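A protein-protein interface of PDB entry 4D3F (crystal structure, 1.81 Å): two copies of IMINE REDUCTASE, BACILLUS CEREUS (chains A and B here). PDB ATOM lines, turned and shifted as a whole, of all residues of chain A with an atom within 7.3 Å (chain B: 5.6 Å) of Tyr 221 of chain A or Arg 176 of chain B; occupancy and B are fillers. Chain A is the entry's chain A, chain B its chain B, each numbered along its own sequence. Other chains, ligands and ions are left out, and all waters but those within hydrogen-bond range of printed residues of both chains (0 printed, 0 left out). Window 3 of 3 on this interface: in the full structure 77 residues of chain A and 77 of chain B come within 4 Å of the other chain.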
ATOM      1  N   ILE A 213      20.349   3.981 -32.091  1.00  0.00           N
ATOM      2  CA  ILE A 213      19.227   4.814 -31.922  1.00  0.00           C
ATOM      3  C   ILE A 213      18.269   4.571 -33.078  1.00  0.00           C
ATOM      4  O   ILE A 213      18.745   4.362 -34.203  1.00  0.00           O
ATOM      5  CB  ILE A 213      19.737   6.309 -31.955  1.00  0.00           C
ATOM      6  CG1 ILE A 213      20.652   6.588 -30.778  1.00  0.00           C
ATOM      7  CG2 ILE A 213      18.608   7.291 -32.012  1.00  0.00           C
ATOM      8  CD1 ILE A 213      20.007   6.252 -29.474  1.00  0.00           C
ATOM      9  N   GLU A 216      12.277   6.299 -34.482  1.00  0.00           N
ATOM     10  CA  GLU A 216      11.324   6.853 -33.519  1.00  0.00           C
ATOM     11  C   GLU A 216      12.008   7.794 -32.498  1.00  0.00           C
ATOM     12  O   GLU A 216      11.470   8.870 -32.212  1.00  0.00           O
ATOM     13  CB  GLU A 216      10.515   5.726 -32.766  1.00  0.00           C
ATOM     14  CG  GLU A 216       9.392   6.304 -31.878  1.00  0.00           C
ATOM     15  CD  GLU A 216       8.223   6.979 -32.602  1.00  0.00           C
ATOM     16  OE1 GLU A 216       8.021   6.760 -33.817  1.00  0.00           O
ATOM     17  OE2 GLU A 216       7.461   7.744 -31.939  1.00  0.00           O
ATOM     18  N   GLN A 217      13.143   7.404 -31.994  1.00  0.00           N
ATOM     19  CA  GLN A 217      13.915   8.208 -31.061  1.00  0.00           C
ATOM     20  C   GLN A 217      14.446   9.534 -31.751  1.00  0.00           C
ATOM     21  O   GLN A 217      14.453  10.616 -31.142  1.00  0.00           O
ATOM     22  CB  GLN A 217      15.075   7.433 -30.522  1.00  0.00           C
ATOM     23  CG  GLN A 217      14.720   6.338 -29.543  1.00  0.00           C
ATOM     24  CD  GLN A 217      15.946   5.589 -29.099  1.00  0.00           C
ATOM     25  OE1 GLN A 217      16.579   4.836 -29.831  1.00  0.00           O
ATOM     26  NE2 GLN A 217      16.326   5.819 -27.870  1.00  0.00           N
ATOM     27  N   PHE A 218      14.885   9.414 -33.022  1.00  0.00           N
ATOM     28  CA  PHE A 218      15.408  10.570 -33.797  1.00  0.00           C
ATOM     29  C   PHE A 218      14.346  11.526 -34.224  1.00  0.00           C
ATOM     30  O   PHE A 218      14.598  12.730 -34.352  1.00  0.00           O
ATOM     31  CB  PHE A 218      16.223  10.048 -34.970  1.00  0.00           C
ATOM     32  CG  PHE A 218      16.995  11.109 -35.756  1.00  0.00           C
ATOM     33  CD1 PHE A 218      17.573  12.236 -35.128  1.00  0.00           C
ATOM     34  CD2 PHE A 218      17.238  10.915 -37.101  1.00  0.00           C
ATOM     35  CE1 PHE A 218      18.260  13.189 -35.839  1.00  0.00           C
ATOM     36  CE2 PHE A 218      17.997  11.847 -37.822  1.00  0.00           C
ATOM     37  CZ  PHE A 218      18.515  12.980 -37.181  1.00  0.00           C
ATOM     38  N   LEU A 219      13.125  11.043 -34.464  1.00  0.00           N
ATOM     39  CA  LEU A 219      12.015  11.859 -34.985  1.00  0.00           C
ATOM     40  C   LEU A 219      11.844  13.265 -34.465  1.00  0.00           C
ATOM     41  O   LEU A 219      11.737  14.214 -35.260  1.00  0.00           O
ATOM     42  CB  LEU A 219      10.677  11.097 -34.871  1.00  0.00           C
ATOM     43  CG  LEU A 219       9.369  11.819 -35.200  1.00  0.00           C
ATOM     44  CD1 LEU A 219       9.353  12.200 -36.666  1.00  0.00           C
ATOM     45  CD2 LEU A 219       8.149  10.968 -34.901  1.00  0.00           C
ATOM     46  N   PRO A 220      11.755  13.456 -33.121  1.00  0.00           N
ATOM     47  CA  PRO A 220      11.497  14.820 -32.704  1.00  0.00           C
ATOM     48  C   PRO A 220      12.699  15.799 -32.988  1.00  0.00           C
ATOM     49  O   PRO A 220      12.460  16.964 -33.195  1.00  0.00           O
ATOM     50  CB  PRO A 220      11.210  14.724 -31.246  1.00  0.00           C
ATOM     51  CG  PRO A 220      11.677  13.392 -30.822  1.00  0.00           C
ATOM     52  CD  PRO A 220      11.673  12.485 -32.013  1.00  0.00           C
ATOM     53  N   TYR A 221      13.875  15.258 -33.044  1.00  0.00           N
ATOM     54  CA  TYR A 221      15.103  16.032 -33.262  1.00  0.00           C
ATOM     55  C   TYR A 221      15.251  16.351 -34.752  1.00  0.00           C
ATOM     56  O   TYR A 221      15.597  17.491 -35.108  1.00  0.00           O
ATOM     57  CB  TYR A 221      16.281  15.236 -32.751  1.00  0.00           C
ATOM     58  CG  TYR A 221      16.118  14.972 -31.255  1.00  0.00           C
ATOM     59  CD1 TYR A 221      16.147  16.012 -30.336  1.00  0.00           C
ATOM     60  CD2 TYR A 221      15.819  13.733 -30.782  1.00  0.00           C
ATOM     61  CE1 TYR A 221      15.984  15.789 -28.967  1.00  0.00           C
ATOM     62  CE2 TYR A 221      15.612  13.531 -29.420  1.00  0.00           C
ATOM     63  CZ  TYR A 221      15.696  14.578 -28.543  1.00  0.00           C
ATOM     64  OH  TYR A 221      15.498  14.345 -27.188  1.00  0.00           O
ATOM     65  N   ALA A 222      15.090  15.336 -35.600  1.00  0.00           N
ATOM     66  CA  ALA A 222      15.060  15.603 -37.074  1.00  0.00           C
ATOM     67  C   ALA A 222      14.017  16.626 -37.415  1.00  0.00           C
ATOM     68  O   ALA A 222      14.291  17.581 -38.168  1.00  0.00           O
ATOM     69  CB  ALA A 222      14.897  14.288 -37.859  1.00  0.00           C
ATOM     70  N   SER A 223      12.800  16.489 -36.890  1.00  0.00           N
ATOM     71  CA  SER A 223      11.731  17.404 -37.150  1.00  0.00           C
ATOM     72  C   SER A 223      11.996  18.788 -36.658  1.00  0.00           C
ATOM     73  O   SER A 223      11.726  19.722 -37.369  1.00  0.00           O
ATOM     74  CB  SER A 223      10.410  16.926 -36.524  1.00  0.00           C
ATOM     75  OG  SER A 223      10.081  15.676 -37.068  1.00  0.00           O
ATOM     76  N   ALA A 224      12.568  18.920 -35.463  1.00  0.00           N
ATOM     77  CA  ALA A 224      12.842  20.229 -34.920  1.00  0.00           C
ATOM     78  C   ALA A 224      13.918  20.922 -35.775  1.00  0.00           C
ATOM     79  O   ALA A 224      13.829  22.131 -36.043  1.00  0.00           O
ATOM     80  CB  ALA A 224      13.342  20.154 -33.473  1.00  0.00           C
ATOM     81  N   MET A 225      14.881  20.153 -36.233  1.00  0.00           N
ATOM     82  CA  MET A 225      15.941  20.789 -37.075  1.00  0.00           C
ATOM     83  C   MET A 225      15.360  21.302 -38.372  1.00  0.00           C
ATOM     84  O   MET A 225      15.655  22.437 -38.776  1.00  0.00           O
ATOM     85  CB  MET A 225      17.064  19.830 -37.303  1.00  0.00           C
ATOM     86  CG  MET A 225      18.152  20.385 -38.212  1.00  0.00           C
ATOM     87  SD  MET A 225      18.868  21.934 -37.643  1.00  0.00           S
ATOM     88  CE  MET A 225      19.970  21.409 -36.322  1.00  0.00           C
ATOM     89  N   MET A 226      14.592  20.450 -39.063  1.00  0.00           N
ATOM     90  CA  MET A 226      13.959  20.866 -40.317  1.00  0.00           C
ATOM     91  C   MET A 226      13.110  22.054 -40.140  1.00  0.00           C
ATOM     92  O   MET A 226      13.142  22.986 -40.925  1.00  0.00           O
ATOM     93  CB  MET A 226      13.167  19.727 -40.922  1.00  0.00           C
ATOM     94  CG  MET A 226      14.103  18.665 -41.416  1.00  0.00           C
ATOM     95  SD  MET A 226      13.300  17.082 -41.617  1.00  0.00           S
ATOM     96  CE  MET A 226      14.613  16.319 -42.588  1.00  0.00           C
ATOM     97  N   SER A 227      12.293  22.074 -39.070  1.00  0.00           N
ATOM     98  CA  SER A 227      11.408  23.194 -38.854  1.00  0.00           C
ATOM     99  C   SER A 227      12.149  24.488 -38.534  1.00  0.00           C
ATOM    100  O   SER A 227      11.529  25.525 -38.630  1.00  0.00           O
ATOM    101  CB  SER A 227      10.357  22.869 -37.707  1.00  0.00           C
ATOM    102  OG  SER A 227       9.495  21.842 -38.166  1.00  0.00           O
ATOM    103  N   TYR B 152      22.108  18.670 -25.092  1.00  0.00           N
ATOM    104  CA  TYR B 152      22.059  17.238 -24.974  1.00  0.00           C
ATOM    105  C   TYR B 152      23.089  16.834 -23.927  1.00  0.00           C
ATOM    106  O   TYR B 152      24.178  17.334 -23.917  1.00  0.00           O
ATOM    107  CB  TYR B 152      22.473  16.523 -26.249  1.00  0.00           C
ATOM    108  CG  TYR B 152      21.613  16.838 -27.438  1.00  0.00           C
ATOM    109  CD1 TYR B 152      20.287  16.434 -27.479  1.00  0.00           C
ATOM    110  CD2 TYR B 152      22.142  17.490 -28.540  1.00  0.00           C
ATOM    111  CE1 TYR B 152      19.527  16.615 -28.607  1.00  0.00           C
ATOM    112  CE2 TYR B 152      21.332  17.773 -29.650  1.00  0.00           C
ATOM    113  CZ  TYR B 152      20.059  17.289 -29.675  1.00  0.00           C
ATOM    114  OH  TYR B 152      19.249  17.591 -30.742  1.00  0.00           O
ATOM    115  N   TYR B 153      22.714  15.932 -23.032  1.00  0.00           N
ATOM    116  CA  TYR B 153      23.629  15.377 -22.057  1.00  0.00           C
ATOM    117  C   TYR B 153      23.610  13.872 -22.061  1.00  0.00           C
ATOM    118  O   TYR B 153      22.585  13.253 -22.340  1.00  0.00           O
ATOM    119  CB  TYR B 153      23.336  15.886 -20.602  1.00  0.00           C
ATOM    120  CG  TYR B 153      23.717  17.316 -20.366  1.00  0.00           C
ATOM    121  CD1 TYR B 153      25.017  17.676 -20.264  1.00  0.00           C
ATOM    122  CD2 TYR B 153      22.748  18.305 -20.279  1.00  0.00           C
ATOM    123  CE1 TYR B 153      25.375  18.968 -20.063  1.00  0.00           C
ATOM    124  CE2 TYR B 153      23.097  19.618 -20.087  1.00  0.00           C
ATOM    125  CZ  TYR B 153      24.424  19.934 -19.983  1.00  0.00           C
ATOM    126  OH  TYR B 153      24.802  21.258 -19.778  1.00  0.00           O
ATOM    127  N   SER B 154      24.756  13.288 -21.806  1.00  0.00           N
ATOM    128  CA  SER B 154      24.841  11.860 -21.652  1.00  0.00           C
ATOM    129  C   SER B 154      26.001  11.473 -20.779  1.00  0.00           C
ATOM    130  O   SER B 154      26.955  12.257 -20.547  1.00  0.00           O
ATOM    131  CB  SER B 154      24.915  11.120 -23.028  1.00  0.00           C
ATOM    132  OG  SER B 154      26.123  11.386 -23.705  1.00  0.00           O
ATOM    133  N   ASP B 174      18.611  18.020 -21.836  1.00  0.00           N
ATOM    134  CA  ASP B 174      17.969  16.858 -22.450  1.00  0.00           C
ATOM    135  C   ASP B 174      18.848  15.664 -22.308  1.00  0.00           C
ATOM    136  O   ASP B 174      19.749  15.400 -23.129  1.00  0.00           O
ATOM    137  CB  ASP B 174      17.596  17.203 -23.922  1.00  0.00           C
ATOM    138  CG  ASP B 174      16.883  16.031 -24.649  1.00  0.00           C
ATOM    139  OD1 ASP B 174      16.657  14.963 -24.028  1.00  0.00           O
ATOM    140  OD2 ASP B 174      16.665  16.166 -25.866  1.00  0.00           O
ATOM    141  N   TYR B 175      18.659  14.910 -21.218  1.00  0.00           N
ATOM    142  CA  TYR B 175      19.496  13.762 -20.914  1.00  0.00           C
ATOM    143  C   TYR B 175      19.118  12.618 -21.876  1.00  0.00           C
ATOM    144  O   TYR B 175      17.978  12.227 -21.935  1.00  0.00           O
ATOM    145  CB  TYR B 175      19.289  13.287 -19.455  1.00  0.00           C
ATOM    146  CG  TYR B 175      20.096  12.061 -19.106  1.00  0.00           C
ATOM    147  CD1 TYR B 175      21.436  12.140 -18.828  1.00  0.00           C
ATOM    148  CD2 TYR B 175      19.494  10.802 -18.988  1.00  0.00           C
ATOM    149  CE1 TYR B 175      22.191  11.022 -18.530  1.00  0.00           C
ATOM    150  CE2 TYR B 175      20.242   9.685 -18.704  1.00  0.00           C
ATOM    151  CZ  TYR B 175      21.562   9.797 -18.423  1.00  0.00           C
ATOM    152  OH  TYR B 175      22.353   8.741 -18.146  1.00  0.00           O
ATOM    153  N   ARG B 176      20.069  12.091 -22.608  1.00  0.00           N
ATOM    154  CA  ARG B 176      19.838  11.126 -23.696  1.00  0.00           C
ATOM    155  C   ARG B 176      20.191   9.675 -23.339  1.00  0.00           C
ATOM    156  O   ARG B 176      19.768   8.767 -24.055  1.00  0.00           O
ATOM    157  CB  ARG B 176      20.620  11.542 -24.990  1.00  0.00           C
ATOM    158  CG  ARG B 176      20.192  12.874 -25.501  1.00  0.00           C
ATOM    159  CD  ARG B 176      18.966  12.779 -26.381  1.00  0.00           C
ATOM    160  NE  ARG B 176      17.817  12.704 -25.619  1.00  0.00           N
ATOM    161  CZ  ARG B 176      16.818  11.850 -25.748  1.00  0.00           C
ATOM    162  NH1 ARG B 176      16.723  10.854 -26.618  1.00  0.00           N
ATOM    163  NH2 ARG B 176      15.871  12.008 -24.916  1.00  0.00           N
ATOM    164  N   GLY B 177      20.885   9.439 -22.234  1.00  0.00           N
ATOM    165  CA  GLY B 177      21.235   8.088 -21.792  1.00  0.00           C
ATOM    166  C   GLY B 177      22.632   7.949 -21.230  1.00  0.00           C
ATOM    167  O   GLY B 177      23.392   8.942 -21.128  1.00  0.00           O
ATOM    168  N   GLU B 178      22.988   6.704 -20.871  1.00  0.00           N
ATOM    169  CA  GLU B 178      24.227   6.412 -20.182  1.00  0.00           C
ATOM    170  C   GLU B 178      25.467   6.491 -21.049  1.00  0.00           C
ATOM    171  O   GLU B 178      26.531   6.784 -20.572  1.00  0.00           O
ATOM    172  CB  GLU B 178      24.220   4.981 -19.515  1.00  0.00           C
ATOM    173  N   LEU B 182      26.424   9.564 -26.648  1.00  0.00           N
ATOM    174  CA  LEU B 182      25.122   9.950 -27.196  1.00  0.00           C
ATOM    175  C   LEU B 182      24.922  11.429 -27.349  1.00  0.00           C
ATOM    176  O   LEU B 182      24.215  11.874 -28.281  1.00  0.00           O
ATOM    177  CB  LEU B 182      23.999   9.408 -26.291  1.00  0.00           C
ATOM    178  CG  LEU B 182      23.262   8.089 -26.528  1.00  0.00           C
ATOM    179  CD1 LEU B 182      23.645   7.264 -27.753  1.00  0.00           C
ATOM    180  CD2 LEU B 182      22.972   7.288 -25.272  1.00  0.00           C
ATOM    181  N   ALA B 183      25.419  12.261 -26.384  1.00  0.00           N
ATOM    182  CA  ALA B 183      25.188  13.668 -26.501  1.00  0.00           C
ATOM    183  C   ALA B 183      25.866  14.202 -27.799  1.00  0.00           C
ATOM    184  O   ALA B 183      25.257  15.032 -28.443  1.00  0.00           O
ATOM    185  CB  ALA B 183      25.729  14.437 -25.309  1.00  0.00           C
ATOM    186  N   TYR B 186      23.597  12.827 -31.033  1.00  0.00           N
ATOM    187  CA  TYR B 186      22.478  13.644 -31.348  1.00  0.00           C
ATOM    188  C   TYR B 186      22.859  15.016 -31.924  1.00  0.00           C
ATOM    189  O   TYR B 186      22.188  15.560 -32.853  1.00  0.00           O
ATOM    190  CB  TYR B 186      21.628  13.828 -30.092  1.00  0.00           C
ATOM    191  CG  TYR B 186      20.714  12.601 -29.730  1.00  0.00           C
ATOM    192  CD1 TYR B 186      21.171  11.549 -28.969  1.00  0.00           C
ATOM    193  CD2 TYR B 186      19.406  12.530 -30.192  1.00  0.00           C
ATOM    194  CE1 TYR B 186      20.354  10.472 -28.647  1.00  0.00           C
ATOM    195  CE2 TYR B 186      18.626  11.426 -29.936  1.00  0.00           C
ATOM    196  CZ  TYR B 186      19.082  10.442 -29.123  1.00  0.00           C
ATOM    197  OH  TYR B 186      18.222   9.388 -28.851  1.00  0.00           O
ATOM    198  N   GLN B 190      22.134  16.045 -36.092  1.00  0.00           N
ATOM    199  CA  GLN B 190      21.399  17.250 -36.394  1.00  0.00           C
ATOM    200  C   GLN B 190      22.226  18.184 -37.266  1.00  0.00           C
ATOM    201  O   GLN B 190      21.681  18.851 -38.142  1.00  0.00           O
ATOM    202  CB  GLN B 190      20.967  17.994 -35.158  1.00  0.00           C
ATOM    203  CG  GLN B 190      19.694  17.433 -34.570  1.00  0.00           C
ATOM    204  CD  GLN B 190      19.135  18.434 -33.537  1.00  0.00           C
ATOM    205  OE1 GLN B 190      19.916  19.118 -32.773  1.00  0.00           O
ATOM    206  NE2 GLN B 190      17.808  18.658 -33.615  1.00  0.00           N
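Of the printed residues of chain A, Asp 174 of chain B touches Tyr 221 (2.5 Å). Arg 176 of chain B touches one residue of chain A. Of the printed residues of chain A, Gln 190 of chain B touches Tyr 221 (2.9 Å) and Met 225 (3.6 Å). The nearest printed residue of chain A that does not touch Tyr 186 of chain B is Gln 217 of chain A (4.1 Å).
Printed residues of chain B that touch a printed residue of chain A: Tyr 152, Asp 174, Arg 176, Tyr 186 and Gln 190. Along chain B the printed residues that touch a printed residue of chain A span positions 152 to 190. Of the 13 printed residues of chain A, 3 touch a printed residue of chain B. Hydrophobic or aromatic side chains of chain A within 4 Å of the printed part of chain B: Ile 213, Tyr 221 and Met 225.
Tyr 186 of chain B touches Ile 213 of chain A. CD1 of Tyr 221 of chain A touches OH of Tyr 152 of chain B, 3.5 Å away. Tyr 186 of chain B touches Tyr 221 of chain A (CE2 to CE2, 3.7 Å). Met 225 of chain A touches Gln 190 of chain B.
The side-chain hydroxyl (OH) of Tyr 152 of chain B lies within hydrogen-bond range of the side-chain amide oxygen (OE1) of Gln 190 of chain B, at 2.6 Å. O of Tyr 153 of chain B is in hydrogen-bond range of N of Arg 176 of chain B, 2.8 Å away. The guanidinium group of Arg 176 of chain B is in salt-bridge range of the side-chain carboxylate of Asp 174 of chain B (3.0 Å). The side-chain hydroxyl of Tyr 186 of chain B sits at hydrogen-bond distance from the guanidinium group of Arg 176 of chain B (3.1 Å). The backbone carbonyl oxygen (O) of Asp 174 of chain B lies within hydrogen-bond range of the backbone NH (N) of Tyr 153 of chain B (3.0 Å).
No position is printed for both chains. Of the 7 pairs that touch across the chains among the printed residues, none has its exchanged pair printed and touching as well.
The side-chain hydroxyl (OH) of Tyr 221 of chain A lies close to the guanidinium group (NE) of Arg 176 of chain B. O of Tyr 221 of chain A sits at hydrogen-bond distance from NE2 of Gln 190 of chain B, at 2.9 Å. The side-chain carboxylate of Asp 174 of chain B sits at hydrogen-bond distance from the side-chain hydroxyl of Tyr 221 of chain A, 2.5 Å away.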
